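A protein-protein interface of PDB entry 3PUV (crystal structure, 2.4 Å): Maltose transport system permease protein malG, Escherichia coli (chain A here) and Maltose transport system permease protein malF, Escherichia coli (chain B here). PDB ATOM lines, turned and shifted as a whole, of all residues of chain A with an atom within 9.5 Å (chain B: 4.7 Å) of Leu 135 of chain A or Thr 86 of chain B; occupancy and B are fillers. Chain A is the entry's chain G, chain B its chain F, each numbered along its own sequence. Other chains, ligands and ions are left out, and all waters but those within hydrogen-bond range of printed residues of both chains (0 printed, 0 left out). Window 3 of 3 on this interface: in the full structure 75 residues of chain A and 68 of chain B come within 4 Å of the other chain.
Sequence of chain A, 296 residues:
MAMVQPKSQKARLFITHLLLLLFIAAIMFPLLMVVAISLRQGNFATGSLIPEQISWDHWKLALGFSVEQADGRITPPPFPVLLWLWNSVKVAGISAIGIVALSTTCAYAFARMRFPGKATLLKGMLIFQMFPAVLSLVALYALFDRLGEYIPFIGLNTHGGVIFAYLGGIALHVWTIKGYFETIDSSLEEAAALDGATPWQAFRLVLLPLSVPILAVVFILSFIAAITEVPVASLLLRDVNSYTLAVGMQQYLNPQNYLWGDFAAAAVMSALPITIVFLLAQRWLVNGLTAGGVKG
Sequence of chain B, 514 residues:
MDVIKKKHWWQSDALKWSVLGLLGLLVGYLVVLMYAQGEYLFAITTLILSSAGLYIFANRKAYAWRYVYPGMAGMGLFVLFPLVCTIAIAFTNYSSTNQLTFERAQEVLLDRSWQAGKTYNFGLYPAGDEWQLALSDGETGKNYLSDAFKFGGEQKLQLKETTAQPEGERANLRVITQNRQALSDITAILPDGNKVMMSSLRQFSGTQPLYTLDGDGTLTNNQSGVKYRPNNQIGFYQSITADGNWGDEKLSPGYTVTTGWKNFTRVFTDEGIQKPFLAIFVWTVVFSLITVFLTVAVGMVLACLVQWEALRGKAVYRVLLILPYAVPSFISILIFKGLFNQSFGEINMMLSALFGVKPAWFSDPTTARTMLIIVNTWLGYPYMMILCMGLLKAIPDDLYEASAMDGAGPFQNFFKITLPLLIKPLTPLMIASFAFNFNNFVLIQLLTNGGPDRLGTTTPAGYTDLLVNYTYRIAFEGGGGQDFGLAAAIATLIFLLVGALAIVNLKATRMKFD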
ATOM      1  N   PHE A 131       0.147  24.274  26.205  1.00  0.00           N
ATOM      2  CA  PHE A 131      -0.769  24.713  25.157  1.00  0.00           C
ATOM      3  C   PHE A 131      -2.214  24.470  25.608  1.00  0.00           C
ATOM      4  O   PHE A 131      -2.500  23.442  26.236  1.00  0.00           O
ATOM      5  CB  PHE A 131      -0.481  23.956  23.854  1.00  0.00           C
ATOM      6  CG  PHE A 131      -1.161  24.539  22.644  1.00  0.00           C
ATOM      7  CD1 PHE A 131      -2.420  24.095  22.251  1.00  0.00           C
ATOM      8  CD2 PHE A 131      -0.536  25.529  21.891  1.00  0.00           C
ATOM      9  CE1 PHE A 131      -3.053  24.638  21.129  1.00  0.00           C
ATOM     10  CE2 PHE A 131      -1.157  26.078  20.768  1.00  0.00           C
ATOM     11  CZ  PHE A 131      -2.417  25.631  20.386  1.00  0.00           C
ATOM     12  N   PRO A 132      -3.128  25.418  25.301  1.00  0.00           N
ATOM     13  CA  PRO A 132      -4.540  25.269  25.662  1.00  0.00           C
ATOM     14  C   PRO A 132      -5.218  24.079  24.976  1.00  0.00           C
ATOM     15  O   PRO A 132      -5.313  24.041  23.743  1.00  0.00           O
ATOM     16  CB  PRO A 132      -5.164  26.589  25.192  1.00  0.00           C
ATOM     17  CG  PRO A 132      -4.038  27.551  25.172  1.00  0.00           C
ATOM     18  CD  PRO A 132      -2.856  26.752  24.733  1.00  0.00           C
ATOM     19  N   ALA A 133      -5.680  23.123  25.783  1.00  0.00           N
ATOM     20  CA  ALA A 133      -6.369  21.924  25.287  1.00  0.00           C
ATOM     21  C   ALA A 133      -7.846  22.192  24.964  1.00  0.00           C
ATOM     22  O   ALA A 133      -8.747  21.571  25.538  1.00  0.00           O
ATOM     23  CB  ALA A 133      -6.222  20.769  26.293  1.00  0.00           C
ATOM     24  N   VAL A 134      -8.083  23.111  24.030  1.00  0.00           N
ATOM     25  CA  VAL A 134      -9.441  23.549  23.685  1.00  0.00           C
ATOM     26  C   VAL A 134     -10.077  22.722  22.551  1.00  0.00           C
ATOM     27  O   VAL A 134     -11.234  22.305  22.655  1.00  0.00           O
ATOM     28  CB  VAL A 134      -9.495  25.090  23.394  1.00  0.00           C
ATOM     29  CG1 VAL A 134      -8.587  25.476  22.227  1.00  0.00           C
ATOM     30  CG2 VAL A 134     -10.932  25.568  23.164  1.00  0.00           C
ATOM     31  N   LEU A 135      -9.316  22.490  21.482  1.00  0.00           N
ATOM     32  CA  LEU A 135      -9.787  21.721  20.328  1.00  0.00           C
ATOM     33  C   LEU A 135      -9.113  20.350  20.262  1.00  0.00           C
ATOM     34  O   LEU A 135      -9.008  19.743  19.195  1.00  0.00           O
ATOM     35  CB  LEU A 135      -9.548  22.504  19.025  1.00  0.00           C
ATOM     36  CG  LEU A 135     -10.581  23.499  18.467  1.00  0.00           C
ATOM     37  CD1 LEU A 135     -11.828  22.787  17.943  1.00  0.00           C
ATOM     38  CD2 LEU A 135     -10.960  24.592  19.466  1.00  0.00           C
ATOM     39  N   SER A 136      -8.667  19.866  21.417  1.00  0.00           N
ATOM     40  CA  SER A 136      -7.920  18.616  21.501  1.00  0.00           C
ATOM     41  C   SER A 136      -8.808  17.376  21.371  1.00  0.00           C
ATOM     42  O   SER A 136      -8.400  16.381  20.769  1.00  0.00           O
ATOM     43  CB  SER A 136      -7.112  18.562  22.800  1.00  0.00           C
ATOM     44  OG  SER A 136      -7.935  18.810  23.927  1.00  0.00           O
ATOM     45  N   LEU A 137     -10.016  17.445  21.929  1.00  0.00           N
ATOM     46  CA  LEU A 137     -10.958  16.319  21.905  1.00  0.00           C
ATOM     47  C   LEU A 137     -11.407  15.938  20.495  1.00  0.00           C
ATOM     48  O   LEU A 137     -11.678  14.767  20.218  1.00  0.00           O
ATOM     49  CB  LEU A 137     -12.175  16.608  22.788  1.00  0.00           C
ATOM     50  CG  LEU A 137     -11.947  16.747  24.299  1.00  0.00           C
ATOM     51  CD1 LEU A 137     -13.256  17.090  24.996  1.00  0.00           C
ATOM     52  CD2 LEU A 137     -11.329  15.490  24.908  1.00  0.00           C
ATOM     53  N   VAL A 138     -11.481  16.933  19.614  1.00  0.00           N
ATOM     54  CA  VAL A 138     -11.735  16.708  18.192  1.00  0.00           C
ATOM     55  C   VAL A 138     -10.622  15.836  17.599  1.00  0.00           C
ATOM     56  O   VAL A 138     -10.893  14.871  16.881  1.00  0.00           O
ATOM     57  CB  VAL A 138     -11.825  18.047  17.414  1.00  0.00           C
ATOM     58  CG1 VAL A 138     -12.195  17.806  15.956  1.00  0.00           C
ATOM     59  CG2 VAL A 138     -12.830  18.987  18.070  1.00  0.00           C
ATOM     60  N   ALA A 139      -9.377  16.178  17.926  1.00  0.00           N
ATOM     61  CA  ALA A 139      -8.208  15.467  17.420  1.00  0.00           C
ATOM     62  C   ALA A 139      -8.048  14.083  18.050  1.00  0.00           C
ATOM     63  O   ALA A 139      -7.646  13.135  17.372  1.00  0.00           O
ATOM     64  CB  ALA A 139      -6.953  16.300  17.630  1.00  0.00           C
ATOM     65  N   LEU A 140      -8.369  13.976  19.338  1.00  0.00           N
ATOM     66  CA  LEU A 140      -8.251  12.717  20.080  1.00  0.00           C
ATOM     67  C   LEU A 140      -9.233  11.642  19.606  1.00  0.00           C
ATOM     68  O   LEU A 140      -8.855  10.478  19.453  1.00  0.00           O
ATOM     69  CB  LEU A 140      -8.402  12.955  21.588  1.00  0.00           C
ATOM     70  CG  LEU A 140      -7.159  13.440  22.349  1.00  0.00           C
ATOM     71  CD1 LEU A 140      -7.544  14.120  23.656  1.00  0.00           C
ATOM     72  CD2 LEU A 140      -6.175  12.300  22.609  1.00  0.00           C
ATOM     73  N   TYR A 141     -10.485  12.036  19.375  1.00  0.00           N
ATOM     74  CA  TYR A 141     -11.509  11.110  18.899  1.00  0.00           C
ATOM     75  C   TYR A 141     -11.124  10.540  17.540  1.00  0.00           C
ATOM     76  O   TYR A 141     -11.220   9.333  17.318  1.00  0.00           O
ATOM     77  CB  TYR A 141     -12.874  11.798  18.823  1.00  0.00           C
ATOM     78  CG  TYR A 141     -14.027  10.861  18.524  1.00  0.00           C
ATOM     79  CD1 TYR A 141     -14.551  10.027  19.515  1.00  0.00           C
ATOM     80  CD2 TYR A 141     -14.603  10.817  17.254  1.00  0.00           C
ATOM     81  CE1 TYR A 141     -15.612   9.167  19.246  1.00  0.00           C
ATOM     82  CE2 TYR A 141     -15.664   9.960  16.974  1.00  0.00           C
ATOM     83  CZ  TYR A 141     -16.165   9.137  17.975  1.00  0.00           C
ATOM     84  OH  TYR A 141     -17.222   8.289  17.706  1.00  0.00           O
ATOM     85  N   ALA A 142     -10.669  11.421  16.650  1.00  0.00           N
ATOM     86  CA  ALA A 142     -10.226  11.042  15.310  1.00  0.00           C
ATOM     87  C   ALA A 142      -9.053  10.062  15.345  1.00  0.00           C
ATOM     88  O   ALA A 142      -8.922   9.216  14.461  1.00  0.00           O
ATOM     89  CB  ALA A 142      -9.860  12.281  14.504  1.00  0.00           C
ATOM     90  N   PRO B  82      -2.539  16.778  18.896  1.00  0.00           N
ATOM     91  CA  PRO B  82      -3.669  17.667  19.184  1.00  0.00           C
ATOM     92  C   PRO B  82      -3.324  19.151  19.069  1.00  0.00           C
ATOM     93  O   PRO B  82      -4.190  19.957  18.731  1.00  0.00           O
ATOM     94  CB  PRO B  82      -4.016  17.326  20.635  1.00  0.00           C
ATOM     95  CG  PRO B  82      -3.591  15.921  20.786  1.00  0.00           C
ATOM     96  CD  PRO B  82      -2.326  15.820  19.998  1.00  0.00           C
ATOM     97  N   LEU B  83      -2.073  19.502  19.352  1.00  0.00           N
ATOM     98  CA  LEU B  83      -1.607  20.879  19.226  1.00  0.00           C
ATOM     99  C   LEU B  83      -1.571  21.326  17.762  1.00  0.00           C
ATOM    100  O   LEU B  83      -1.980  22.444  17.445  1.00  0.00           O
ATOM    101  CB  LEU B  83      -0.233  21.038  19.892  1.00  0.00           C
ATOM    102  CG  LEU B  83       0.592  22.314  19.706  1.00  0.00           C
ATOM    103  CD1 LEU B  83       1.405  22.583  20.953  1.00  0.00           C
ATOM    104  CD2 LEU B  83       1.506  22.213  18.489  1.00  0.00           C
ATOM    105  N   VAL B  84      -1.082  20.451  16.884  1.00  0.00           N
ATOM    106  CA  VAL B  84      -0.961  20.759  15.457  1.00  0.00           C
ATOM    107  C   VAL B  84      -2.338  20.966  14.822  1.00  0.00           C
ATOM    108  O   VAL B  84      -2.533  21.914  14.059  1.00  0.00           O
ATOM    109  CB  VAL B  84      -0.154  19.671  14.692  1.00  0.00           C
ATOM    110  CG1 VAL B  84      -0.092  19.979  13.199  1.00  0.00           C
ATOM    111  CG2 VAL B  84       1.256  19.548  15.255  1.00  0.00           C
ATOM    112  N   CYS B  85      -3.283  20.089  15.161  1.00  0.00           N
ATOM    113  CA  CYS B  85      -4.657  20.158  14.654  1.00  0.00           C
ATOM    114  C   CYS B  85      -5.361  21.460  15.015  1.00  0.00           C
ATOM    115  O   CYS B  85      -5.983  22.085  14.156  1.00  0.00           O
ATOM    116  CB  CYS B  85      -5.479  18.973  15.163  1.00  0.00           C
ATOM    117  SG  CYS B  85      -4.962  17.384  14.494  1.00  0.00           S
ATOM    118  N   THR B  86      -5.262  21.855  16.283  1.00  0.00           N
ATOM    119  CA  THR B  86      -5.819  23.122  16.763  1.00  0.00           C
ATOM    120  C   THR B  86      -5.307  24.293  15.923  1.00  0.00           C
ATOM    121  O   THR B  86      -6.091  25.127  15.465  1.00  0.00           O
ATOM    122  CB  THR B  86      -5.499  23.345  18.262  1.00  0.00           C
ATOM    123  OG1 THR B  86      -6.184  22.359  19.043  1.00  0.00           O
ATOM    124  CG2 THR B  86      -5.943  24.729  18.727  1.00  0.00           C
ATOM    125  N   ILE B  87      -3.992  24.332  15.715  1.00  0.00           N
ATOM    126  CA  ILE B  87      -3.357  25.337  14.869  1.00  0.00           C
ATOM    127  C   ILE B  87      -3.845  25.207  13.424  1.00  0.00           C
ATOM    128  O   ILE B  87      -4.189  26.207  12.794  1.00  0.00           O
ATOM    129  CB  ILE B  87      -1.806  25.256  14.953  1.00  0.00           C
ATOM    130  CG1 ILE B  87      -1.338  25.598  16.374  1.00  0.00           C
ATOM    131  CG2 ILE B  87      -1.146  26.189  13.932  1.00  0.00           C
ATOM    132  CD1 ILE B  87       0.113  25.262  16.664  1.00  0.00           C
ATOM    133  N   ALA B  88      -3.896  23.976  12.916  1.00  0.00           N
ATOM    134  CA  ALA B  88      -4.368  23.712  11.556  1.00  0.00           C
ATOM    135  C   ALA B  88      -5.790  24.227  11.335  1.00  0.00           C
ATOM    136  O   ALA B  88      -6.067  24.882  10.330  1.00  0.00           O
ATOM    137  CB  ALA B  88      -4.276  22.224  11.228  1.00  0.00           C
ATOM    138  N   ILE B  89      -6.674  23.941  12.292  1.00  0.00           N
ATOM    139  CA  ILE B  89      -8.073  24.378  12.245  1.00  0.00           C
ATOM    140  C   ILE B  89      -8.209  25.907  12.264  1.00  0.00           C
ATOM    141  O   ILE B  89      -9.176  26.453  11.727  1.00  0.00           O
ATOM    142  CB  ILE B  89      -8.912  23.703  13.373  1.00  0.00           C
ATOM    143  CG1 ILE B  89      -9.249  22.259  12.980  1.00  0.00           C
ATOM    144  CG2 ILE B  89     -10.199  24.481  13.669  1.00  0.00           C
ATOM    145  CD1 ILE B  89      -9.730  21.382  14.129  1.00  0.00           C
ATOM    146  N   ALA B  90      -7.224  26.587  12.852  1.00  0.00           N
ATOM    147  CA  ALA B  90      -7.226  28.051  12.953  1.00  0.00           C
ATOM    148  C   ALA B  90      -7.150  28.767  11.601  1.00  0.00           C
ATOM    149  O   ALA B  90      -7.487  29.949  11.503  1.00  0.00           O
ATOM    150  CB  ALA B  90      -6.107  28.522  13.871  1.00  0.00           C
ATOM    151  N   PHE B 484     -15.241  27.375  15.968  1.00  0.00           N
ATOM    152  CA  PHE B 484     -14.060  26.633  16.405  1.00  0.00           C
ATOM    153  C   PHE B 484     -12.787  27.205  15.793  1.00  0.00           C
ATOM    154  O   PHE B 484     -11.720  27.147  16.405  1.00  0.00           O
ATOM    155  CB  PHE B 484     -14.186  25.144  16.060  1.00  0.00           C
ATOM    156  CG  PHE B 484     -15.432  24.491  16.598  1.00  0.00           C
ATOM    157  CD1 PHE B 484     -16.415  24.029  15.732  1.00  0.00           C
ATOM    158  CD2 PHE B 484     -15.618  24.334  17.967  1.00  0.00           C
ATOM    159  CE1 PHE B 484     -17.567  23.422  16.218  1.00  0.00           C
ATOM    160  CE2 PHE B 484     -16.770  23.731  18.464  1.00  0.00           C
ATOM    161  CZ  PHE B 484     -17.746  23.274  17.587  1.00  0.00           C
ATOM    162  N   ALA B 487     -11.855  30.267  17.930  1.00  0.00           N
ATOM    163  CA  ALA B 487     -11.345  29.816  19.227  1.00  0.00           C
ATOM    164  C   ALA B 487      -9.964  29.175  19.125  1.00  0.00           C
ATOM    165  O   ALA B 487      -9.170  29.260  20.061  1.00  0.00           O
ATOM    166  CB  ALA B 487     -12.324  28.856  19.882  1.00  0.00           C
ATOM    167  N   ALA B 488      -9.692  28.531  17.991  1.00  0.00           N
ATOM    168  CA  ALA B 488      -8.396  27.909  17.741  1.00  0.00           C
ATOM    169  C   ALA B 488      -7.317  28.963  17.495  1.00  0.00           C
ATOM    170  O   ALA B 488      -6.185  28.817  17.958  1.00  0.00           O
ATOM    171  CB  ALA B 488      -8.484  26.956  16.565  1.00  0.00           C
ATOM    172  N   ALA B 491      -6.569  30.664  20.731  1.00  0.00           N
ATOM    173  CA  ALA B 491      -5.800  29.705  21.527  1.00  0.00           C
ATOM    174  C   ALA B 491      -4.319  29.730  21.148  1.00  0.00           C
ATOM    175  O   ALA B 491      -3.447  29.603  22.012  1.00  0.00           O
ATOM    176  CB  ALA B 491      -6.363  28.304  21.373  1.00  0.00           C
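O of Ala 133 of chain A sits at hydrogen-bond distance from OG of Ser 136 of chain A (3.3 Å).
The backbone carbonyl oxygen (O) of Pro 82 of chain B sits at hydrogen-bond distance from the side-chain hydroxyl (OG1) of Thr 86 of chain B (3.1 Å).
Of the printed residues of chain B, Phe 131 of chain A touches Leu 83 (3.6 Å) and Thr 86 (3.8 Å).
Of the printed residues of chain B, Val 134 of chain A touches Ala 491 (3.7 Å).
Of chain B, only Thr 86 (3.4 Å) and Phe 484 (3.8 Å) come within 4 Å of Leu 135 of chain A.
Printed residues of chain B within 4 Å of Ser 136 of chain A: Pro 82 (3.97 Å).
Of the printed residues of chain B, Ala 139 of chain A touches Pro 82 and Cys 85.
Printed residues of chain A within 4 Å of Leu 83 of chain B: Phe 131 (3.6 Å).
Cys 85 of chain B touches one residue of chain A.
Thr 86 of chain B touches two residues of chain A.
Ala 88 of chain B touches none of the printed residues of chain A.
No residue of chain A comes within 4 Å of Ile 89 of chain B.
The nearest residue of chain A that does not touch Thr 86 of chain B is Ser 136 of chain A (4.2 Å).
Among the printed residues, merely in contact across the chains: Phe 131 of chain A with Leu 83 of chain B (3.6 Å), Phe 131 of chain A with Thr 86 of chain B (3.8 Å), Pro 132 of chain A with Ala 491 of chain B (3.8 Å), Val 134 of chain A with Ala 491 of chain B (3.7 Å), Leu 135 of chain A with Thr 86 of chain B (3.4 Å), Leu 135 of chain A with Phe 484 of chain B (3.8 Å), Ser 136 of chain A with Pro 82 of chain B (3.97 Å), Ala 139 of chain A with Pro 82 of chain B (3.9 Å) and Ala 139 of chain A with Cys 85 of chain B (3.9 Å).
Among the printed residues, 9 pairs touch across the chains.
Among the printed residues, no Asp or Glu carboxylate lies within 4 Å of a Lys or Arg side-chain nitrogen of the other chain.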
